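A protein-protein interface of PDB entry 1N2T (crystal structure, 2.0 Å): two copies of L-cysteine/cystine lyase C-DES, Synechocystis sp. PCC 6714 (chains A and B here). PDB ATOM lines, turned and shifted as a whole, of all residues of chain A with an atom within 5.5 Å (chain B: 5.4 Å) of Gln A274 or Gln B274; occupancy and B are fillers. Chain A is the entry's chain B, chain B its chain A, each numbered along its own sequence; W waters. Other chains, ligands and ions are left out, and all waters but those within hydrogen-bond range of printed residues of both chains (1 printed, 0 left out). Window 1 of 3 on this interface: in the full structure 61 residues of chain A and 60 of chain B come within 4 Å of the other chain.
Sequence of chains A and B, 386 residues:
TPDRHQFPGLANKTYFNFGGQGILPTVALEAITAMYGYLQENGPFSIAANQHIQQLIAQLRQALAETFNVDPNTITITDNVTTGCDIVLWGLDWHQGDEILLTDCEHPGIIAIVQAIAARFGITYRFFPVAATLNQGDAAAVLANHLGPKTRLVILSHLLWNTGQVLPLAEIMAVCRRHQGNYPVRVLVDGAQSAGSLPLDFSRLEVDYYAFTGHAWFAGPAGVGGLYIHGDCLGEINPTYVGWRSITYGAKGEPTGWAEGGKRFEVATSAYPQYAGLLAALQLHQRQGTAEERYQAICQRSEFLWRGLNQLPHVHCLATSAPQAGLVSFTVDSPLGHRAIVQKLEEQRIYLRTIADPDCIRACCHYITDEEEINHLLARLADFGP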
ATOM      1  N   ILE A  32      -9.686   0.436  28.801  1.00  0.00           N
ATOM      2  CA  ILE A  32     -10.369   0.503  27.510  1.00  0.00           C
ATOM      3  C   ILE A  32     -11.339   1.688  27.557  1.00  0.00           C
ATOM      4  O   ILE A  32     -11.326   2.553  26.689  1.00  0.00           O
ATOM      5  CB  ILE A  32     -11.137  -0.814  27.238  1.00  0.00           C
ATOM      6  CG1 ILE A  32     -10.121  -1.939  26.971  1.00  0.00           C
ATOM      7  CG2 ILE A  32     -12.122  -0.631  26.075  1.00  0.00           C
ATOM      8  CD1 ILE A  32     -10.685  -3.363  27.040  1.00  0.00           C
ATOM      9  N   TYR A  36     -11.358   5.479  25.253  1.00  0.00           N
ATOM     10  CA  TYR A  36     -12.462   6.007  24.445  1.00  0.00           C
ATOM     11  C   TYR A  36     -12.743   7.418  24.908  1.00  0.00           C
ATOM     12  O   TYR A  36     -13.005   8.299  24.103  1.00  0.00           O
ATOM     13  CB  TYR A  36     -13.725   5.160  24.604  1.00  0.00           C
ATOM     14  CG  TYR A  36     -13.752   3.947  23.716  1.00  0.00           C
ATOM     15  CD1 TYR A  36     -13.745   2.666  24.258  1.00  0.00           C
ATOM     16  CD2 TYR A  36     -13.776   4.079  22.322  1.00  0.00           C
ATOM     17  CE1 TYR A  36     -13.759   1.535  23.435  1.00  0.00           C
ATOM     18  CE2 TYR A  36     -13.788   2.966  21.497  1.00  0.00           C
ATOM     19  CZ  TYR A  36     -13.779   1.702  22.057  1.00  0.00           C
ATOM     20  OH  TYR A  36     -13.784   0.619  21.228  1.00  0.00           O
ATOM     21  N   PRO A 221      -8.371  -8.389  26.151  1.00  0.00           N
ATOM     22  CA  PRO A 221      -9.611  -8.466  25.382  1.00  0.00           C
ATOM     23  C   PRO A 221      -9.432  -9.157  24.025  1.00  0.00           C
ATOM     24  O   PRO A 221      -8.339  -9.166  23.478  1.00  0.00           O
ATOM     25  CB  PRO A 221      -9.991  -7.003  25.217  1.00  0.00           C
ATOM     26  CG  PRO A 221      -8.660  -6.325  25.083  1.00  0.00           C
ATOM     27  CD  PRO A 221      -7.781  -7.039  26.098  1.00  0.00           C
ATOM     28  N   ALA A 222     -10.511  -9.719  23.487  1.00  0.00           N
ATOM     29  CA  ALA A 222     -10.476 -10.350  22.170  1.00  0.00           C
ATOM     30  C   ALA A 222     -10.059  -9.284  21.151  1.00  0.00           C
ATOM     31  O   ALA A 222     -10.572  -8.160  21.186  1.00  0.00           O
ATOM     32  CB  ALA A 222     -11.842 -10.876  21.816  1.00  0.00           C
ATOM     33  N   VAL A 224      -6.450  -8.530  20.271  1.00  0.00           N
ATOM     34  CA  VAL A 224      -5.062  -8.093  20.303  1.00  0.00           C
ATOM     35  C   VAL A 224      -4.133  -9.288  20.567  1.00  0.00           C
ATOM     36  O   VAL A 224      -4.330 -10.017  21.539  1.00  0.00           O
ATOM     37  CB  VAL A 224      -4.817  -7.041  21.412  1.00  0.00           C
ATOM     38  CG1 VAL A 224      -3.398  -6.454  21.267  1.00  0.00           C
ATOM     39  CG2 VAL A 224      -5.863  -5.935  21.335  1.00  0.00           C
ATOM     40  N   ALA A 271      -7.988  -1.369  16.748  1.00  0.00           N
ATOM     41  CA  ALA A 271      -8.799  -1.008  17.914  1.00  0.00           C
ATOM     42  C   ALA A 271      -7.911  -0.578  19.080  1.00  0.00           C
ATOM     43  O   ALA A 271      -7.750  -1.309  20.058  1.00  0.00           O
ATOM     44  CB  ALA A 271      -9.654  -2.193  18.315  1.00  0.00           C
ATOM     45  N   TYR A 272      -7.372   0.637  18.983  1.00  0.00           N
ATOM     46  CA  TYR A 272      -6.440   1.156  19.983  1.00  0.00           C
ATOM     47  C   TYR A 272      -6.840   1.024  21.442  1.00  0.00           C
ATOM     48  O   TYR A 272      -5.990   0.703  22.277  1.00  0.00           O
ATOM     49  CB  TYR A 272      -6.093   2.621  19.665  1.00  0.00           C
ATOM     50  CG  TYR A 272      -5.644   2.821  18.229  1.00  0.00           C
ATOM     51  CD1 TYR A 272      -6.246   3.783  17.413  1.00  0.00           C
ATOM     52  CD2 TYR A 272      -4.641   2.027  17.676  1.00  0.00           C
ATOM     53  CE1 TYR A 272      -5.857   3.948  16.063  1.00  0.00           C
ATOM     54  CE2 TYR A 272      -4.240   2.185  16.338  1.00  0.00           C
ATOM     55  CZ  TYR A 272      -4.856   3.149  15.537  1.00  0.00           C
ATOM     56  OH  TYR A 272      -4.467   3.319  14.211  1.00  0.00           O
ATOM     57  N   PRO A 273      -8.116   1.292  21.780  1.00  0.00           N
ATOM     58  CA  PRO A 273      -8.546   1.171  23.180  1.00  0.00           C
ATOM     59  C   PRO A 273      -8.257  -0.220  23.734  1.00  0.00           C
ATOM     60  O   PRO A 273      -7.919  -0.360  24.905  1.00  0.00           O
ATOM     61  CB  PRO A 273     -10.053   1.452  23.110  1.00  0.00           C
ATOM     62  CG  PRO A 273     -10.162   2.421  21.993  1.00  0.00           C
ATOM     63  CD  PRO A 273      -9.207   1.829  20.942  1.00  0.00           C
ATOM     64  N   GLN A 274      -8.402  -1.241  22.892  1.00  0.00           N
ATOM     65  CA  GLN A 274      -8.151  -2.623  23.309  1.00  0.00           C
ATOM     66  C   GLN A 274      -6.684  -2.837  23.634  1.00  0.00           C
ATOM     67  O   GLN A 274      -6.344  -3.666  24.484  1.00  0.00           O
ATOM     68  CB  GLN A 274      -8.599  -3.616  22.222  1.00  0.00           C
ATOM     69  CG  GLN A 274     -10.090  -4.007  22.288  1.00  0.00           C
ATOM     70  CD  GLN A 274     -10.990  -2.835  22.011  1.00  0.00           C
ATOM     71  OE1 GLN A 274     -12.065  -2.693  22.615  1.00  0.00           O
ATOM     72  NE2 GLN A 274     -10.565  -1.972  21.087  1.00  0.00           N
ATOM     73  N   TYR A 275      -5.813  -2.084  22.966  1.00  0.00           N
ATOM     74  CA  TYR A 275      -4.374  -2.200  23.215  1.00  0.00           C
ATOM     75  C   TYR A 275      -4.113  -1.796  24.664  1.00  0.00           C
ATOM     76  O   TYR A 275      -3.267  -2.377  25.335  1.00  0.00           O
ATOM     77  CB  TYR A 275      -3.569  -1.257  22.304  1.00  0.00           C
ATOM     78  CG  TYR A 275      -3.364  -1.685  20.852  1.00  0.00           C
ATOM     79  CD1 TYR A 275      -2.444  -1.014  20.052  1.00  0.00           C
ATOM     80  CD2 TYR A 275      -4.088  -2.728  20.276  1.00  0.00           C
ATOM     81  CE1 TYR A 275      -2.238  -1.363  18.711  1.00  0.00           C
ATOM     82  CE2 TYR A 275      -3.890  -3.083  18.925  1.00  0.00           C
ATOM     83  CZ  TYR A 275      -2.964  -2.393  18.155  1.00  0.00           C
ATOM     84  OH  TYR A 275      -2.756  -2.707  16.831  1.00  0.00           O
ATOM     85  N   ALA A 276      -4.825  -0.775  25.133  1.00  0.00           N
ATOM     86  CA  ALA A 276      -4.671  -0.308  26.509  1.00  0.00           C
ATOM     87  C   ALA A 276      -5.195  -1.373  27.472  1.00  0.00           C
ATOM     88  O   ALA A 276      -4.708  -1.512  28.596  1.00  0.00           O
ATOM     89  CB  ALA A 276      -5.424   0.988  26.711  1.00  0.00           C
ATOM     90  N   GLY A 277      -6.208  -2.114  27.044  1.00  0.00           N
ATOM     91  CA  GLY A 277      -6.725  -3.164  27.899  1.00  0.00           C
ATOM     92  C   GLY A 277      -5.682  -4.263  28.083  1.00  0.00           C
ATOM     93  O   GLY A 277      -5.452  -4.718  29.211  1.00  0.00           O
ATOM     94  N   LEU A 278      -5.041  -4.697  26.996  1.00  0.00           N
ATOM     95  CA  LEU A 278      -4.037  -5.754  27.109  1.00  0.00           C
ATOM     96  C   LEU A 278      -2.855  -5.274  27.946  1.00  0.00           C
ATOM     97  O   LEU A 278      -2.313  -6.022  28.762  1.00  0.00           O
ATOM     98  CB  LEU A 278      -3.529  -6.192  25.734  1.00  0.00           C
ATOM     99  CG  LEU A 278      -2.390  -7.228  25.814  1.00  0.00           C
ATOM    100  CD1 LEU A 278      -2.845  -8.434  26.623  1.00  0.00           C
ATOM    101  CD2 LEU A 278      -1.975  -7.661  24.411  1.00  0.00           C
ATOM    102  N   LEU A 279      -2.437  -4.027  27.729  1.00  0.00           N
ATOM    103  CA  LEU A 279      -1.334  -3.496  28.501  1.00  0.00           C
ATOM    104  C   LEU A 279      -1.658  -3.582  30.001  1.00  0.00           C
ATOM    105  O   LEU A 279      -0.820  -3.999  30.789  1.00  0.00           O
ATOM    106  CB  LEU A 279      -1.053  -2.051  28.100  1.00  0.00           C
ATOM    107  CG  LEU A 279      -0.005  -1.288  28.920  1.00  0.00           C
ATOM    108  CD1 LEU A 279       1.359  -1.972  28.801  1.00  0.00           C
ATOM    109  CD2 LEU A 279       0.083   0.158  28.408  1.00  0.00           C
ATOM    110  N   ILE B  32     -20.732  -1.180  22.713  1.00  0.00           N
ATOM    111  CA  ILE B  32     -19.419  -1.718  22.997  1.00  0.00           C
ATOM    112  C   ILE B  32     -19.363  -2.160  24.457  1.00  0.00           C
ATOM    113  O   ILE B  32     -19.002  -3.302  24.766  1.00  0.00           O
ATOM    114  CB  ILE B  32     -18.344  -0.653  22.695  1.00  0.00           C
ATOM    115  CG1 ILE B  32     -18.226  -0.495  21.176  1.00  0.00           C
ATOM    116  CG2 ILE B  32     -17.006  -1.069  23.291  1.00  0.00           C
ATOM    117  CD1 ILE B  32     -17.519   0.760  20.711  1.00  0.00           C
ATOM    118  N   TYR B  36     -19.021  -6.188  26.268  1.00  0.00           N
ATOM    119  CA  TYR B  36     -18.052  -6.636  27.265  1.00  0.00           C
ATOM    120  C   TYR B  36     -18.810  -7.244  28.451  1.00  0.00           C
ATOM    121  O   TYR B  36     -18.406  -8.276  28.994  1.00  0.00           O
ATOM    122  CB  TYR B  36     -17.201  -5.477  27.760  1.00  0.00           C
ATOM    123  CG  TYR B  36     -16.068  -5.132  26.826  1.00  0.00           C
ATOM    124  CD1 TYR B  36     -16.020  -3.897  26.192  1.00  0.00           C
ATOM    125  CD2 TYR B  36     -15.044  -6.043  26.580  1.00  0.00           C
ATOM    126  CE1 TYR B  36     -14.983  -3.569  25.332  1.00  0.00           C
ATOM    127  CE2 TYR B  36     -13.994  -5.727  25.721  1.00  0.00           C
ATOM    128  CZ  TYR B  36     -13.971  -4.498  25.105  1.00  0.00           C
ATOM    129  OH  TYR B  36     -12.960  -4.141  24.249  1.00  0.00           O
ATOM    130  N   PRO B 221     -16.230   2.775  15.669  1.00  0.00           N
ATOM    131  CA  PRO B 221     -14.957   2.837  16.392  1.00  0.00           C
ATOM    132  C   PRO B 221     -13.800   2.403  15.512  1.00  0.00           C
ATOM    133  O   PRO B 221     -14.008   1.678  14.534  1.00  0.00           O
ATOM    134  CB  PRO B 221     -15.174   1.854  17.559  1.00  0.00           C
ATOM    135  CG  PRO B 221     -16.046   0.799  16.924  1.00  0.00           C
ATOM    136  CD  PRO B 221     -17.042   1.629  16.127  1.00  0.00           C
ATOM    137  N   ALA B 222     -12.586   2.837  15.863  1.00  0.00           N
ATOM    138  CA  ALA B 222     -11.392   2.422  15.122  1.00  0.00           C
ATOM    139  C   ALA B 222     -11.267   0.900  15.251  1.00  0.00           C
ATOM    140  O   ALA B 222     -11.464   0.343  16.331  1.00  0.00           O
ATOM    141  CB  ALA B 222     -10.126   3.095  15.709  1.00  0.00           C
ATOM    142  N   VAL B 224     -12.751  -1.480  12.758  1.00  0.00           N
ATOM    143  CA  VAL B 224     -13.698  -2.294  12.001  1.00  0.00           C
ATOM    144  C   VAL B 224     -13.938  -1.679  10.623  1.00  0.00           C
ATOM    145  O   VAL B 224     -14.253  -0.491  10.523  1.00  0.00           O
ATOM    146  CB  VAL B 224     -15.073  -2.425  12.722  1.00  0.00           C
ATOM    147  CG1 VAL B 224     -15.938  -3.462  11.981  1.00  0.00           C
ATOM    148  CG2 VAL B 224     -14.895  -2.832  14.178  1.00  0.00           C
ATOM    149  N   ALA B 271     -12.000  -7.974  17.500  1.00  0.00           N
ATOM    150  CA  ALA B 271     -12.565  -7.169  18.578  1.00  0.00           C
ATOM    151  C   ALA B 271     -14.097  -7.104  18.454  1.00  0.00           C
ATOM    152  O   ALA B 271     -14.649  -6.088  18.029  1.00  0.00           O
ATOM    153  CB  ALA B 271     -11.975  -5.775  18.523  1.00  0.00           C
ATOM    154  N   TYR B 272     -14.773  -8.184  18.842  1.00  0.00           N
ATOM    155  CA  TYR B 272     -16.231  -8.278  18.730  1.00  0.00           C
ATOM    156  C   TYR B 272     -17.038  -7.118  19.315  1.00  0.00           C
ATOM    157  O   TYR B 272     -17.986  -6.661  18.703  1.00  0.00           O
ATOM    158  CB  TYR B 272     -16.706  -9.629  19.306  1.00  0.00           C
ATOM    159  CG  TYR B 272     -15.928 -10.823  18.761  1.00  0.00           C
ATOM    160  CD1 TYR B 272     -15.379 -11.768  19.614  1.00  0.00           C
ATOM    161  CD2 TYR B 272     -15.737 -10.992  17.388  1.00  0.00           C
ATOM    162  CE1 TYR B 272     -14.649 -12.856  19.114  1.00  0.00           C
ATOM    163  CE2 TYR B 272     -15.025 -12.065  16.887  1.00  0.00           C
ATOM    164  CZ  TYR B 272     -14.481 -12.996  17.749  1.00  0.00           C
ATOM    165  OH  TYR B 272     -13.778 -14.057  17.231  1.00  0.00           O
ATOM    166  N   PRO B 273     -16.669  -6.611  20.505  1.00  0.00           N
ATOM    167  CA  PRO B 273     -17.460  -5.495  21.044  1.00  0.00           C
ATOM    168  C   PRO B 273     -17.485  -4.301  20.079  1.00  0.00           C
ATOM    169  O   PRO B 273     -18.474  -3.551  20.000  1.00  0.00           O
ATOM    170  CB  PRO B 273     -16.746  -5.161  22.351  1.00  0.00           C
ATOM    171  CG  PRO B 273     -16.146  -6.526  22.765  1.00  0.00           C
ATOM    172  CD  PRO B 273     -15.609  -7.025  21.447  1.00  0.00           C
ATOM    173  N   GLN B 274     -16.393  -4.105  19.352  1.00  0.00           N
ATOM    174  CA  GLN B 274     -16.332  -3.003  18.392  1.00  0.00           C
ATOM    175  C   GLN B 274     -17.254  -3.231  17.197  1.00  0.00           C
ATOM    176  O   GLN B 274     -17.694  -2.277  16.574  1.00  0.00           O
ATOM    177  CB  GLN B 274     -14.903  -2.780  17.892  1.00  0.00           C
ATOM    178  CG  GLN B 274     -14.058  -1.942  18.838  1.00  0.00           C
ATOM    179  CD  GLN B 274     -13.803  -2.615  20.166  1.00  0.00           C
ATOM    180  OE1 GLN B 274     -13.683  -1.942  21.198  1.00  0.00           O
ATOM    181  NE2 GLN B 274     -13.701  -3.941  20.157  1.00  0.00           N
ATOM    182  N   TYR B 275     -17.508  -4.494  16.865  1.00  0.00           N
ATOM    183  CA  TYR B 275     -18.420  -4.822  15.778  1.00  0.00           C
ATOM    184  C   TYR B 275     -19.823  -4.293  16.146  1.00  0.00           C
ATOM    185  O   TYR B 275     -20.554  -3.783  15.291  1.00  0.00           O
ATOM    186  CB  TYR B 275     -18.518  -6.337  15.590  1.00  0.00           C
ATOM    187  CG  TYR B 275     -17.402  -7.020  14.825  1.00  0.00           C
ATOM    188  CD1 TYR B 275     -17.566  -8.333  14.370  1.00  0.00           C
ATOM    189  CD2 TYR B 275     -16.188  -6.388  14.572  1.00  0.00           C
ATOM    190  CE1 TYR B 275     -16.550  -9.003  13.682  1.00  0.00           C
ATOM    191  CE2 TYR B 275     -15.158  -7.053  13.882  1.00  0.00           C
ATOM    192  CZ  TYR B 275     -15.354  -8.361  13.442  1.00  0.00           C
ATOM    193  OH  TYR B 275     -14.359  -9.031  12.766  1.00  0.00           O
ATOM    194  N   ALA B 276     -20.198  -4.450  17.417  1.00  0.00           N
ATOM    195  CA  ALA B 276     -21.501  -3.995  17.910  1.00  0.00           C
ATOM    196  C   ALA B 276     -21.544  -2.474  17.862  1.00  0.00           C
ATOM    197  O   ALA B 276     -22.598  -1.868  17.634  1.00  0.00           O
ATOM    198  CB  ALA B 276     -21.716  -4.474  19.349  1.00  0.00           C
ATOM    199  N   GLY B 277     -20.385  -1.856  18.078  1.00  0.00           N
ATOM    200  CA  GLY B 277     -20.309  -0.403  18.049  1.00  0.00           C
ATOM    201  C   GLY B 277     -20.617   0.096  16.641  1.00  0.00           C
ATOM    202  O   GLY B 277     -21.423   1.014  16.465  1.00  0.00           O
ATOM    203  N   LEU B 278     -19.961  -0.493  15.639  1.00  0.00           N
ATOM    204  CA  LEU B 278     -20.201  -0.100  14.245  1.00  0.00           C
ATOM    205  C   LEU B 278     -21.662  -0.351  13.861  1.00  0.00           C
ATOM    206  O   LEU B 278     -22.288   0.481  13.198  1.00  0.00           O
ATOM    207  CB  LEU B 278     -19.321  -0.894  13.270  1.00  0.00           C
ATOM    208  CG  LEU B 278     -19.621  -0.558  11.788  1.00  0.00           C
ATOM    209  CD1 LEU B 278     -19.481   0.935  11.574  1.00  0.00           C
ATOM    210  CD2 LEU B 278     -18.662  -1.311  10.866  1.00  0.00           C
ATOM    211  N   LEU B 279     -22.196  -1.512  14.245  1.00  0.00           N
ATOM    212  CA  LEU B 279     -23.589  -1.818  13.920  1.00  0.00           C
ATOM    213  C   LEU B 279     -24.506  -0.725  14.462  1.00  0.00           C
ATOM    214  O   LEU B 279     -25.404  -0.259  13.759  1.00  0.00           O
ATOM    215  CB  LEU B 279     -24.001  -3.179  14.498  1.00  0.00           C
ATOM    216  CG  LEU B 279     -25.466  -3.599  14.335  1.00  0.00           C
ATOM    217  CD1 LEU B 279     -25.800  -3.732  12.858  1.00  0.00           C
ATOM    218  CD2 LEU B 279     -25.702  -4.943  15.066  1.00  0.00           C
HETATM  219  O   HOH W   1     -11.855   1.424  18.834  1.00  0.00           O
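Gln A274 touches just these residues of chain B: Tyr B36 (2.4 Å) and Gln B274 (2.3 Å). Gln B274 touches two residues of chain A. Printed residues of chain A within 4 Å of Ile B32: Tyr A36. Of the printed residues of chain B, Ala A271 touches Ala B222. Of the printed residues of chain B, Tyr A36 touches Ile B32 (3.8 Å) and Gln B274 (2.6 Å). Of the printed residues of chain B, Ala A222 touches Ala B271. Of the printed residues of chain A, Ala B222 touches Ala A271 (3.4 Å). The nearest residue of chain B that does not touch Gln A274 is Ala B271 (4.6 Å). The nearest residue of chain A that does not touch Gln B274 is Ala A271 (4.4 Å).
Printed residues of chain B that touch a printed residue of chain A: Ile B32, Tyr B36, Ala B222, Ala B271 and Gln B274. Printed residues of chain A that touch a printed residue of chain B: Ile A32, Tyr A36, Ala A222, Ala A271 and Gln A274.
O of Ala B271 lies close to NE2 of Gln B274, 3.2 Å away. The side-chain amide nitrogen (NE2) of Gln A274 lies close to the backbone carbonyl oxygen (O) of Ala A271 (3.1 Å).
Ile A32 touches Tyr B36, and with the chains exchanged Tyr A36 touches Ile B32. Tyr A36 touches Gln B274, and with the chains exchanged Gln A274 touches Tyr B36. Ala A222 touches Ala B271, and with the chains exchanged Ala A271 touches Ala B222. Gln B274 touches its own counterpart, Gln A274. Positions printed for both chains: 32, 36, 221, 222, 224, 271, 272, 273, 274, 275, 276, 277, 278 and 279. Of the 7 pairs that touch across the chains among the printed residues, 7 have their exchanged pair printed and touching as well.
OH of Tyr A36 is in hydrogen-bond range of OE1 of Gln B274, at 2.6 Å. The side-chain amide oxygen (OE1) of Gln B274 sits close to the side-chain amide nitrogen (NE2) of Gln A274 (3.1 Å). The side-chain hydroxyl (OH) of Tyr B36 lies close to the side-chain amide oxygen (OE1) of Gln A274 (2.4 Å).
Water W1 lies within hydrogen-bond range of the backbone carbonyl oxygen (O) of Ala B222 (2.8 Å) and the side-chain hydroxyl (OH) of Tyr A36 (3.2 Å).
Among the printed residues, merely in contact across the chains: Ile A32 with Tyr B36, Tyr A36 with Ile B32, Ala A222 with Ala B271 and Ala A271 with Ala B222.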
